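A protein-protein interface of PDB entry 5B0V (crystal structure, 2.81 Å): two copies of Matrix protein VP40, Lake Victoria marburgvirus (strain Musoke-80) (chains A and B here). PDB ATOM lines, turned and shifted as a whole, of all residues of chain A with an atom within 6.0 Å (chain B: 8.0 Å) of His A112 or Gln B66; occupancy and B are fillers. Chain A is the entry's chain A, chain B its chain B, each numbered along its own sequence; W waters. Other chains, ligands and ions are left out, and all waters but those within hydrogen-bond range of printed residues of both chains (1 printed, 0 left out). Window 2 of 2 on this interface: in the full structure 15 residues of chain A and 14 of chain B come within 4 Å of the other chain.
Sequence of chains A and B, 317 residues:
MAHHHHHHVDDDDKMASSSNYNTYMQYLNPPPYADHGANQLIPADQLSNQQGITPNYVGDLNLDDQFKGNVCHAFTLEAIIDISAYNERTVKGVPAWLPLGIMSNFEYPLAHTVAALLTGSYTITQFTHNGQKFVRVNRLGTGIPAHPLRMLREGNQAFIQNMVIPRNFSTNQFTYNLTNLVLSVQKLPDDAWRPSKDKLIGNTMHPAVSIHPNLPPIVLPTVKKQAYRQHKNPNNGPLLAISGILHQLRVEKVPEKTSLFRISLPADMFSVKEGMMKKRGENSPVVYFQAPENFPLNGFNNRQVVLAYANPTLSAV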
ATOM      1  N   TYR A 108      16.358 -23.330   0.226  1.00  0.00           N
ATOM      2  CA  TYR A 108      15.451 -22.323   0.794  1.00  0.00           C
ATOM      3  C   TYR A 108      15.696 -22.144   2.273  1.00  0.00           C
ATOM      4  O   TYR A 108      15.968 -23.124   2.954  1.00  0.00           O
ATOM      5  CB  TYR A 108      14.004 -22.763   0.576  1.00  0.00           C
ATOM      6  CG  TYR A 108      13.069 -21.602   0.481  1.00  0.00           C
ATOM      7  CD1 TYR A 108      12.475 -21.081   1.608  1.00  0.00           C
ATOM      8  CD2 TYR A 108      12.815 -20.993  -0.738  1.00  0.00           C
ATOM      9  CE1 TYR A 108      11.633 -19.994   1.535  1.00  0.00           C
ATOM     10  CE2 TYR A 108      11.980 -19.904  -0.825  1.00  0.00           C
ATOM     11  CZ  TYR A 108      11.397 -19.411   0.320  1.00  0.00           C
ATOM     12  OH  TYR A 108      10.554 -18.326   0.261  1.00  0.00           O
ATOM     13  N   PRO A 109      15.572 -20.907   2.806  1.00  0.00           N
ATOM     14  CA  PRO A 109      15.787 -20.803   4.264  1.00  0.00           C
ATOM     15  C   PRO A 109      14.996 -21.872   5.032  1.00  0.00           C
ATOM     16  O   PRO A 109      13.773 -21.986   4.897  1.00  0.00           O
ATOM     17  CB  PRO A 109      15.279 -19.406   4.609  1.00  0.00           C
ATOM     18  CG  PRO A 109      15.410 -18.637   3.366  1.00  0.00           C
ATOM     19  CD  PRO A 109      15.252 -19.599   2.211  1.00  0.00           C
ATOM     20  N   LEU A 110      15.705 -22.636   5.842  1.00  0.00           N
ATOM     21  CA  LEU A 110      15.113 -23.691   6.627  1.00  0.00           C
ATOM     22  C   LEU A 110      14.005 -23.220   7.591  1.00  0.00           C
ATOM     23  O   LEU A 110      12.944 -23.831   7.653  1.00  0.00           O
ATOM     24  CB  LEU A 110      16.221 -24.389   7.407  1.00  0.00           C
ATOM     25  CG  LEU A 110      15.895 -25.626   8.236  1.00  0.00           C
ATOM     26  CD1 LEU A 110      15.213 -26.665   7.364  1.00  0.00           C
ATOM     27  CD2 LEU A 110      17.174 -26.182   8.885  1.00  0.00           C
ATOM     28  N   ALA A 111      14.251 -22.160   8.356  1.00  0.00           N
ATOM     29  CA  ALA A 111      13.314 -21.730   9.397  1.00  0.00           C
ATOM     30  C   ALA A 111      11.983 -21.331   8.806  1.00  0.00           C
ATOM     31  O   ALA A 111      10.928 -21.699   9.316  1.00  0.00           O
ATOM     32  CB  ALA A 111      13.883 -20.583  10.205  1.00  0.00           C
ATOM     33  N   HIS A 112      12.013 -20.574   7.731  1.00  0.00           N
ATOM     34  CA  HIS A 112      10.780 -20.282   7.013  1.00  0.00           C
ATOM     35  C   HIS A 112      10.096 -21.573   6.612  1.00  0.00           C
ATOM     36  O   HIS A 112       8.921 -21.768   6.837  1.00  0.00           O
ATOM     37  CB  HIS A 112      11.075 -19.441   5.769  1.00  0.00           C
ATOM     38  CG  HIS A 112       9.863 -18.810   5.177  1.00  0.00           C
ATOM     39  ND1 HIS A 112       9.945 -17.798   4.250  1.00  0.00           N
ATOM     40  CD2 HIS A 112       8.543 -19.013   5.399  1.00  0.00           C
ATOM     41  CE1 HIS A 112       8.727 -17.411   3.915  1.00  0.00           C
ATOM     42  NE2 HIS A 112       7.857 -18.137   4.596  1.00  0.00           N
ATOM     43  N   THR A 113      10.857 -22.478   6.027  1.00  0.00           N
ATOM     44  CA  THR A 113      10.289 -23.727   5.537  1.00  0.00           C
ATOM     45  C   THR A 113       9.562 -24.463   6.653  1.00  0.00           C
ATOM     46  O   THR A 113       8.410 -24.858   6.502  1.00  0.00           O
ATOM     47  CB  THR A 113      11.371 -24.647   4.928  1.00  0.00           C
ATOM     48  OG1 THR A 113      12.076 -23.948   3.885  1.00  0.00           O
ATOM     49  CG2 THR A 113      10.727 -25.886   4.376  1.00  0.00           C
ATOM     50  N   VAL A 114      10.248 -24.618   7.779  1.00  0.00           N
ATOM     51  CA  VAL A 114       9.694 -25.338   8.906  1.00  0.00           C
ATOM     52  C   VAL A 114       8.529 -24.579   9.559  1.00  0.00           C
ATOM     53  O   VAL A 114       7.517 -25.175   9.941  1.00  0.00           O
ATOM     54  CB  VAL A 114      10.777 -25.648   9.950  1.00  0.00           C
ATOM     55  CG1 VAL A 114      10.155 -26.300  11.188  1.00  0.00           C
ATOM     56  CG2 VAL A 114      11.843 -26.548   9.335  1.00  0.00           C
ATOM     57  N   ALA A 115       8.664 -23.269   9.678  1.00  0.00           N
ATOM     58  CA  ALA A 115       7.601 -22.466  10.269  1.00  0.00           C
ATOM     59  C   ALA A 115       6.366 -22.515   9.389  1.00  0.00           C
ATOM     60  O   ALA A 115       5.241 -22.637   9.880  1.00  0.00           O
ATOM     61  CB  ALA A 115       8.065 -21.038  10.446  1.00  0.00           C
ATOM     62  N   ALA A 116       6.595 -22.436   8.082  1.00  0.00           N
ATOM     63  CA  ALA A 116       5.514 -22.455   7.118  1.00  0.00           C
ATOM     64  C   ALA A 116       4.752 -23.787   7.190  1.00  0.00           C
ATOM     65  O   ALA A 116       3.533 -23.840   7.045  1.00  0.00           O
ATOM     66  CB  ALA A 116       6.062 -22.220   5.732  1.00  0.00           C
ATOM     67  N   LEU A 117       5.481 -24.867   7.411  1.00  0.00           N
ATOM     68  CA  LEU A 117       4.877 -26.189   7.395  1.00  0.00           C
ATOM     69  C   LEU A 117       4.059 -26.377   8.656  1.00  0.00           C
ATOM     70  O   LEU A 117       2.898 -26.746   8.592  1.00  0.00           O
ATOM     71  CB  LEU A 117       5.956 -27.278   7.245  1.00  0.00           C
ATOM     72  CG  LEU A 117       6.455 -27.535   5.806  1.00  0.00           C
ATOM     73  CD1 LEU A 117       7.660 -28.455   5.803  1.00  0.00           C
ATOM     74  CD2 LEU A 117       5.354 -28.109   4.924  1.00  0.00           C
ATOM     75  N   ILE A 144       4.051 -20.454  -1.253  1.00  0.00           N
ATOM     76  CA  ILE A 144       5.210 -19.613  -1.508  1.00  0.00           C
ATOM     77  C   ILE A 144       5.986 -20.001  -2.750  1.00  0.00           C
ATOM     78  O   ILE A 144       6.474 -21.126  -2.937  1.00  0.00           O
ATOM     79  CB  ILE A 144       6.145 -19.424  -0.311  1.00  0.00           C
ATOM     80  CG1 ILE A 144       6.455 -20.753   0.347  1.00  0.00           C
ATOM     81  CG2 ILE A 144       5.484 -18.465   0.695  1.00  0.00           C
ATOM     82  CD1 ILE A 144       7.252 -20.621   1.629  1.00  0.00           C
ATOM     83  N   HIS A 147       9.157 -22.475  -4.103  1.00  0.00           N
ATOM     84  CA  HIS A 147       9.616 -23.296  -3.010  1.00  0.00           C
ATOM     85  C   HIS A 147       9.856 -24.718  -3.473  1.00  0.00           C
ATOM     86  O   HIS A 147       9.019 -25.280  -4.148  1.00  0.00           O
ATOM     87  CB  HIS A 147       8.649 -23.305  -1.838  1.00  0.00           C
ATOM     88  CG  HIS A 147       9.310 -23.750  -0.581  1.00  0.00           C
ATOM     89  ND1 HIS A 147       9.729 -25.046  -0.386  1.00  0.00           N
ATOM     90  CD2 HIS A 147       9.747 -23.054   0.489  1.00  0.00           C
ATOM     91  CE1 HIS A 147      10.350 -25.145   0.770  1.00  0.00           C
ATOM     92  NE2 HIS A 147      10.361 -23.951   1.329  1.00  0.00           N
ATOM     93  N   LEU A 152       4.374 -26.396  -0.076  1.00  0.00           N
ATOM     94  CA  LEU A 152       4.454 -24.960   0.205  1.00  0.00           C
ATOM     95  C   LEU A 152       4.368 -24.194  -1.061  1.00  0.00           C
ATOM     96  O   LEU A 152       3.713 -23.166  -1.098  1.00  0.00           O
ATOM     97  CB  LEU A 152       5.752 -24.592   0.882  1.00  0.00           C
ATOM     98  CG  LEU A 152       6.015 -25.241   2.241  1.00  0.00           C
ATOM     99  CD1 LEU A 152       7.393 -24.867   2.754  1.00  0.00           C
ATOM    100  CD2 LEU A 152       4.969 -24.809   3.229  1.00  0.00           C
ATOM    101  N   LEU B  61      -0.659 -15.157  12.749  1.00  0.00           N
ATOM    102  CA  LEU B  61       0.651 -14.709  12.312  1.00  0.00           C
ATOM    103  C   LEU B  61       0.816 -14.920  10.825  1.00  0.00           C
ATOM    104  O   LEU B  61       0.337 -15.905  10.263  1.00  0.00           O
ATOM    105  CB  LEU B  61       1.785 -15.366  13.087  1.00  0.00           C
ATOM    106  CG  LEU B  61       2.540 -16.562  12.538  1.00  0.00           C
ATOM    107  CD1 LEU B  61       3.645 -16.037  11.652  1.00  0.00           C
ATOM    108  CD2 LEU B  61       3.131 -17.363  13.689  1.00  0.00           C
ATOM    109  N   ASN B  62       1.488 -13.957  10.200  1.00  0.00           N
ATOM    110  CA  ASN B  62       1.757 -13.994   8.779  1.00  0.00           C
ATOM    111  C   ASN B  62       3.257 -13.934   8.550  1.00  0.00           C
ATOM    112  O   ASN B  62       3.893 -12.913   8.797  1.00  0.00           O
ATOM    113  CB  ASN B  62       1.053 -12.836   8.098  1.00  0.00           C
ATOM    114  CG  ASN B  62       1.117 -12.917   6.592  1.00  0.00           C
ATOM    115  OD1 ASN B  62       2.004 -13.563   6.019  1.00  0.00           O
ATOM    116  ND2 ASN B  62       0.179 -12.244   5.927  1.00  0.00           N
ATOM    117  N   LEU B  63       3.819 -15.038   8.085  1.00  0.00           N
ATOM    118  CA  LEU B  63       5.246 -15.127   7.862  1.00  0.00           C
ATOM    119  C   LEU B  63       5.735 -14.218   6.753  1.00  0.00           C
ATOM    120  O   LEU B  63       6.886 -13.782   6.766  1.00  0.00           O
ATOM    121  CB  LEU B  63       5.615 -16.547   7.523  1.00  0.00           C
ATOM    122  CG  LEU B  63       5.469 -17.454   8.733  1.00  0.00           C
ATOM    123  CD1 LEU B  63       5.381 -18.916   8.303  1.00  0.00           C
ATOM    124  CD2 LEU B  63       6.638 -17.250   9.674  1.00  0.00           C
ATOM    125  N   ASP B  64       4.866 -13.915   5.795  1.00  0.00           N
ATOM    126  CA  ASP B  64       5.221 -12.982   4.728  1.00  0.00           C
ATOM    127  C   ASP B  64       5.584 -11.602   5.270  1.00  0.00           C
ATOM    128  O   ASP B  64       6.243 -10.819   4.595  1.00  0.00           O
ATOM    129  CB  ASP B  64       4.090 -12.879   3.702  1.00  0.00           C
ATOM    130  CG  ASP B  64       3.817 -14.204   2.988  1.00  0.00           C
ATOM    131  OD1 ASP B  64       4.729 -15.063   2.875  1.00  0.00           O
ATOM    132  OD2 ASP B  64       2.666 -14.373   2.531  1.00  0.00           O
ATOM    133  N   ASP B  65       5.161 -11.294   6.488  1.00  0.00           N
ATOM    134  CA  ASP B  65       5.578 -10.065   7.132  1.00  0.00           C
ATOM    135  C   ASP B  65       6.787 -10.234   8.030  1.00  0.00           C
ATOM    136  O   ASP B  65       7.118  -9.303   8.760  1.00  0.00           O
ATOM    137  CB  ASP B  65       4.445  -9.495   7.963  1.00  0.00           C
ATOM    138  CG  ASP B  65       3.245  -9.121   7.127  1.00  0.00           C
ATOM    139  OD1 ASP B  65       3.416  -8.581   5.998  1.00  0.00           O
ATOM    140  OD2 ASP B  65       2.114  -9.370   7.627  1.00  0.00           O
ATOM    141  N   GLN B  66       7.480 -11.370   7.978  1.00  0.00           N
ATOM    142  CA  GLN B  66       8.668 -11.558   8.838  1.00  0.00           C
ATOM    143  C   GLN B  66       9.716 -10.426   8.738  1.00  0.00           C
ATOM    144  O   GLN B  66      10.473 -10.189   9.682  1.00  0.00           O
ATOM    145  CB  GLN B  66       9.351 -12.895   8.565  1.00  0.00           C
ATOM    146  CG  GLN B  66       9.925 -13.019   7.182  1.00  0.00           C
ATOM    147  CD  GLN B  66      10.491 -14.369   6.928  1.00  0.00           C
ATOM    148  OE1 GLN B  66      11.156 -14.949   7.773  1.00  0.00           O
ATOM    149  NE2 GLN B  66      10.234 -14.881   5.753  1.00  0.00           N
ATOM    150  N   PHE B  67       9.766  -9.748   7.594  1.00  0.00           N
ATOM    151  CA  PHE B  67      10.725  -8.665   7.405  1.00  0.00           C
ATOM    152  C   PHE B  67      10.185  -7.274   7.719  1.00  0.00           C
ATOM    153  O   PHE B  67      10.884  -6.299   7.494  1.00  0.00           O
ATOM    154  CB  PHE B  67      11.276  -8.742   5.988  1.00  0.00           C
ATOM    155  CG  PHE B  67      11.895 -10.071   5.683  1.00  0.00           C
ATOM    156  CD1 PHE B  67      12.833 -10.616   6.547  1.00  0.00           C
ATOM    157  CD2 PHE B  67      11.519 -10.794   4.565  1.00  0.00           C
ATOM    158  CE1 PHE B  67      13.408 -11.841   6.284  1.00  0.00           C
ATOM    159  CE2 PHE B  67      12.085 -12.028   4.299  1.00  0.00           C
ATOM    160  CZ  PHE B  67      13.035 -12.552   5.163  1.00  0.00           C
ATOM    161  N   LYS B  68       8.952  -7.185   8.210  1.00  0.00           N
ATOM    162  CA  LYS B  68       8.419  -5.937   8.709  1.00  0.00           C
ATOM    163  C   LYS B  68       8.690  -5.922  10.180  1.00  0.00           C
ATOM    164  O   LYS B  68       7.996  -6.569  10.947  1.00  0.00           O
ATOM    165  CB  LYS B  68       6.923  -5.808   8.436  1.00  0.00           C
ATOM    166  CG  LYS B  68       6.633  -5.607   6.967  1.00  0.00           C
ATOM    167  CD  LYS B  68       5.200  -5.921   6.561  1.00  0.00           C
ATOM    168  CE  LYS B  68       5.183  -6.351   5.087  1.00  0.00           C
ATOM    169  NZ  LYS B  68       3.875  -6.153   4.410  1.00  0.00           N
ATOM    170  N   GLY B  69       9.710  -5.162  10.561  1.00  0.00           N
ATOM    171  CA  GLY B  69      10.253  -5.188  11.907  1.00  0.00           C
ATOM    172  C   GLY B  69       9.314  -4.656  12.963  1.00  0.00           C
ATOM    173  O   GLY B  69       9.486  -4.938  14.149  1.00  0.00           O
ATOM    174  N   ASN B  70       8.321  -3.894  12.519  1.00  0.00           N
ATOM    175  CA  ASN B  70       7.372  -3.241  13.400  1.00  0.00           C
ATOM    176  C   ASN B  70       6.054  -4.013  13.546  1.00  0.00           C
ATOM    177  O   ASN B  70       4.998  -3.428  13.821  1.00  0.00           O
ATOM    178  CB  ASN B  70       7.084  -1.832  12.866  1.00  0.00           C
ATOM    179  CG  ASN B  70       6.372  -1.854  11.522  1.00  0.00           C
ATOM    180  OD1 ASN B  70       6.623  -2.736  10.674  1.00  0.00           O
ATOM    181  ND2 ASN B  70       5.473  -0.891  11.319  1.00  0.00           N
ATOM    182  N   VAL B  71       6.111  -5.328  13.399  1.00  0.00           N
ATOM    183  CA  VAL B  71       4.963  -6.160  13.689  1.00  0.00           C
ATOM    184  C   VAL B  71       5.254  -6.888  14.993  1.00  0.00           C
ATOM    185  O   VAL B  71       6.352  -7.427  15.161  1.00  0.00           O
ATOM    186  CB  VAL B  71       4.725  -7.115  12.530  1.00  0.00           C
ATOM    187  CG1 VAL B  71       3.589  -8.066  12.830  1.00  0.00           C
ATOM    188  CG2 VAL B  71       4.433  -6.311  11.273  1.00  0.00           C
ATOM    189  N   HIS B  73       4.162  -9.741  17.992  1.00  0.00           N
ATOM    190  CA  HIS B  73       3.356 -10.875  18.320  1.00  0.00           C
ATOM    191  C   HIS B  73       3.398 -11.113  19.798  1.00  0.00           C
ATOM    192  O   HIS B  73       4.428 -10.926  20.434  1.00  0.00           O
ATOM    193  CB  HIS B  73       3.834 -12.088  17.543  1.00  0.00           C
ATOM    194  CG  HIS B  73       3.601 -11.961  16.070  1.00  0.00           C
ATOM    195  ND1 HIS B  73       4.606 -11.662  15.179  1.00  0.00           N
ATOM    196  CD2 HIS B  73       2.463 -12.036  15.342  1.00  0.00           C
ATOM    197  CE1 HIS B  73       4.098 -11.574  13.965  1.00  0.00           C
ATOM    198  NE2 HIS B  73       2.800 -11.796  14.033  1.00  0.00           N
ATOM    199  N   SER B 104       8.692  -7.949  18.910  1.00  0.00           N
ATOM    200  CA  SER B 104       8.533  -7.371  17.596  1.00  0.00           C
ATOM    201  C   SER B 104       9.523  -8.029  16.652  1.00  0.00           C
ATOM    202  O   SER B 104      10.602  -8.480  17.054  1.00  0.00           O
ATOM    203  CB  SER B 104       8.741  -5.868  17.651  1.00  0.00           C
ATOM    204  OG  SER B 104      10.011  -5.571  18.218  1.00  0.00           O
ATOM    205  N   ASN B 105       9.168  -8.065  15.381  1.00  0.00           N
ATOM    206  CA  ASN B 105       9.979  -8.759  14.411  1.00  0.00           C
ATOM    207  C   ASN B 105      11.426  -8.325  14.370  1.00  0.00           C
ATOM    208  O   ASN B 105      12.297  -9.157  14.112  1.00  0.00           O
ATOM    209  CB  ASN B 105       9.334  -8.678  13.031  1.00  0.00           C
ATOM    210  CG  ASN B 105       8.075  -9.529  12.930  1.00  0.00           C
ATOM    211  OD1 ASN B 105       7.812 -10.380  13.775  1.00  0.00           O
ATOM    212  ND2 ASN B 105       7.300  -9.309  11.887  1.00  0.00           N
ATOM    213  N   PHE B 106      11.716  -7.058  14.641  1.00  0.00           N
ATOM    214  CA  PHE B 106      13.107  -6.618  14.571  1.00  0.00           C
ATOM    215  C   PHE B 106      13.964  -7.181  15.683  1.00  0.00           C
ATOM    216  O   PHE B 106      15.175  -7.172  15.562  1.00  0.00           O
ATOM    217  CB  PHE B 106      13.250  -5.093  14.523  1.00  0.00           C
ATOM    218  CG  PHE B 106      12.932  -4.422  15.812  1.00  0.00           C
ATOM    219  CD1 PHE B 106      13.858  -4.406  16.859  1.00  0.00           C
ATOM    220  CD2 PHE B 106      11.695  -3.796  15.988  1.00  0.00           C
ATOM    221  CE1 PHE B 106      13.543  -3.788  18.065  1.00  0.00           C
ATOM    222  CE2 PHE B 106      11.373  -3.170  17.180  1.00  0.00           C
ATOM    223  CZ  PHE B 106      12.298  -3.170  18.226  1.00  0.00           C
ATOM    224  N   TYR B 108      14.323 -10.264  16.720  1.00  0.00           N
ATOM    225  CA  TYR B 108      14.922 -11.544  16.348  1.00  0.00           C
ATOM    226  C   TYR B 108      14.207 -12.127  15.131  1.00  0.00           C
ATOM    227  O   TYR B 108      12.992 -12.012  15.037  1.00  0.00           O
ATOM    228  CB  TYR B 108      14.814 -12.544  17.502  1.00  0.00           C
ATOM    229  CG  TYR B 108      15.929 -13.544  17.480  1.00  0.00           C
ATOM    230  CD1 TYR B 108      15.795 -14.736  16.787  1.00  0.00           C
ATOM    231  CD2 TYR B 108      17.121 -13.297  18.143  1.00  0.00           C
ATOM    232  CE1 TYR B 108      16.829 -15.654  16.753  1.00  0.00           C
ATOM    233  CE2 TYR B 108      18.154 -14.218  18.122  1.00  0.00           C
ATOM    234  CZ  TYR B 108      18.005 -15.387  17.425  1.00  0.00           C
ATOM    235  OH  TYR B 108      19.029 -16.293  17.389  1.00  0.00           O
ATOM    236  N   PRO B 109      14.940 -12.786  14.208  1.00  0.00           N
ATOM    237  CA  PRO B 109      14.224 -13.350  13.065  1.00  0.00           C
ATOM    238  C   PRO B 109      12.997 -14.170  13.496  1.00  0.00           C
ATOM    239  O   PRO B 109      13.098 -15.080  14.330  1.00  0.00           O
ATOM    240  CB  PRO B 109      15.257 -14.249  12.413  1.00  0.00           C
ATOM    241  CG  PRO B 109      16.562 -13.678  12.790  1.00  0.00           C
ATOM    242  CD  PRO B 109      16.392 -13.031  14.122  1.00  0.00           C
ATOM    243  N   LEU B 110      11.849 -13.812  12.944  1.00  0.00           N
ATOM    244  CA  LEU B 110      10.585 -14.432  13.299  1.00  0.00           C
ATOM    245  C   LEU B 110      10.543 -15.912  12.986  1.00  0.00           C
ATOM    246  O   LEU B 110      10.130 -16.701  13.836  1.00  0.00           O
ATOM    247  CB  LEU B 110       9.466 -13.717  12.566  1.00  0.00           C
ATOM    248  CG  LEU B 110       8.034 -14.125  12.814  1.00  0.00           C
ATOM    249  CD1 LEU B 110       7.732 -14.028  14.295  1.00  0.00           C
ATOM    250  CD2 LEU B 110       7.055 -13.258  12.007  1.00  0.00           C
ATOM    251  N   ALA B 111      10.990 -16.304  11.797  1.00  0.00           N
ATOM    252  CA  ALA B 111      10.888 -17.697  11.380  1.00  0.00           C
ATOM    253  C   ALA B 111      11.674 -18.621  12.294  1.00  0.00           C
ATOM    254  O   ALA B 111      11.193 -19.676  12.691  1.00  0.00           O
ATOM    255  CB  ALA B 111      11.342 -17.871   9.937  1.00  0.00           C
ATOM    256  N   HIS B 112      12.902 -18.243  12.613  1.00  0.00           N
ATOM    257  CA  HIS B 112      13.676 -18.993  13.601  1.00  0.00           C
ATOM    258  C   HIS B 112      12.854 -19.080  14.901  1.00  0.00           C
ATOM    259  O   HIS B 112      12.675 -20.148  15.467  1.00  0.00           O
ATOM    260  CB  HIS B 112      15.043 -18.319  13.859  1.00  0.00           C
ATOM    261  CG  HIS B 112      16.017 -19.177  14.603  1.00  0.00           C
ATOM    262  ND1 HIS B 112      17.351 -18.850  14.729  1.00  0.00           N
ATOM    263  CD2 HIS B 112      15.851 -20.351  15.267  1.00  0.00           C
ATOM    264  CE1 HIS B 112      17.965 -19.784  15.437  1.00  0.00           C
ATOM    265  NE2 HIS B 112      17.076 -20.704  15.779  1.00  0.00           N
ATOM    266  N   VAL B 114       9.676 -18.849  15.583  1.00  0.00           N
ATOM    267  CA  VAL B 114       8.508 -19.712  15.492  1.00  0.00           C
ATOM    268  C   VAL B 114       8.904 -21.177  15.271  1.00  0.00           C
ATOM    269  O   VAL B 114       8.303 -22.075  15.851  1.00  0.00           O
ATOM    270  CB  VAL B 114       7.567 -19.233  14.382  1.00  0.00           C
ATOM    271  CG1 VAL B 114       6.411 -20.205  14.199  1.00  0.00           C
ATOM    272  CG2 VAL B 114       7.061 -17.828  14.694  1.00  0.00           C
ATOM    273  N   ALA B 115       9.914 -21.418  14.448  1.00  0.00           N
ATOM    274  CA  ALA B 115      10.360 -22.770  14.186  1.00  0.00           C
ATOM    275  C   ALA B 115      10.926 -23.367  15.454  1.00  0.00           C
ATOM    276  O   ALA B 115      10.669 -24.529  15.770  1.00  0.00           O
ATOM    277  CB  ALA B 115      11.413 -22.782  13.083  1.00  0.00           C
HETATM  278  O   HOH W   1       5.077 -17.601   4.050  1.00  0.00           O
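ND1 of His A112 is in hydrogen-bond range of NE2 of Gln B66 (3.3 Å).
Among the printed residues, pairs that only touch across the chains: Ala A111 with Ala B111, Ala A111 with His B112, Ala A111 with Ala B115, His A112 with Ala B111, Ala A115 with Leu B63 and Ala A116 with Leu B63.
Of the printed residues of chain B, His A112 touches Gln B66 and Ala B111.
Of chain A, only His A112 (3.3 Å) comes within 4 Å of Gln B66.
Of chain B, only Ala B111 (3.6 Å), His B112 (3.5 Å) and Ala B115 (3.9 Å) come within 4 Å of Ala A111.
Printed residues of chain A within 4 Å of Ala B115: Ala A111.
Of the printed residues of chain A, Ala B111 touches Ala A111 (3.6 Å) and His A112 (3.6 Å).
Of the printed residues of chain B, Ala A116 touches Leu B63 (3.7 Å).
The nearest printed residue of chain A that does not touch Ala B111 is Ala A115 (4.1 Å).
Hydrophobic or aromatic side chains of chain A within 4 Å of the printed part of chain B: Ala A111 and His A112.
Of the 22 printed residues of chain B, 5 touch a printed residue of chain A.
Among the printed residues, 7 pairs touch across the chains.
Ala B111 touches its own counterpart, Ala A111.
Ala A111 touches His B112, and with the chains exchanged His A112 touches Ala B111.
Ala A111 touches Ala B115, but with the chains exchanged Ala A115 does not touch Ala B111 (4.1 Å).
Of the 7 pairs that touch across the chains among the printed residues, 3 have their exchanged pair printed and touching as well.
Water W1 lies within hydrogen-bond range of the side-chain carboxylate of Asp B64 and a ring nitrogen (NE2) of His A112.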
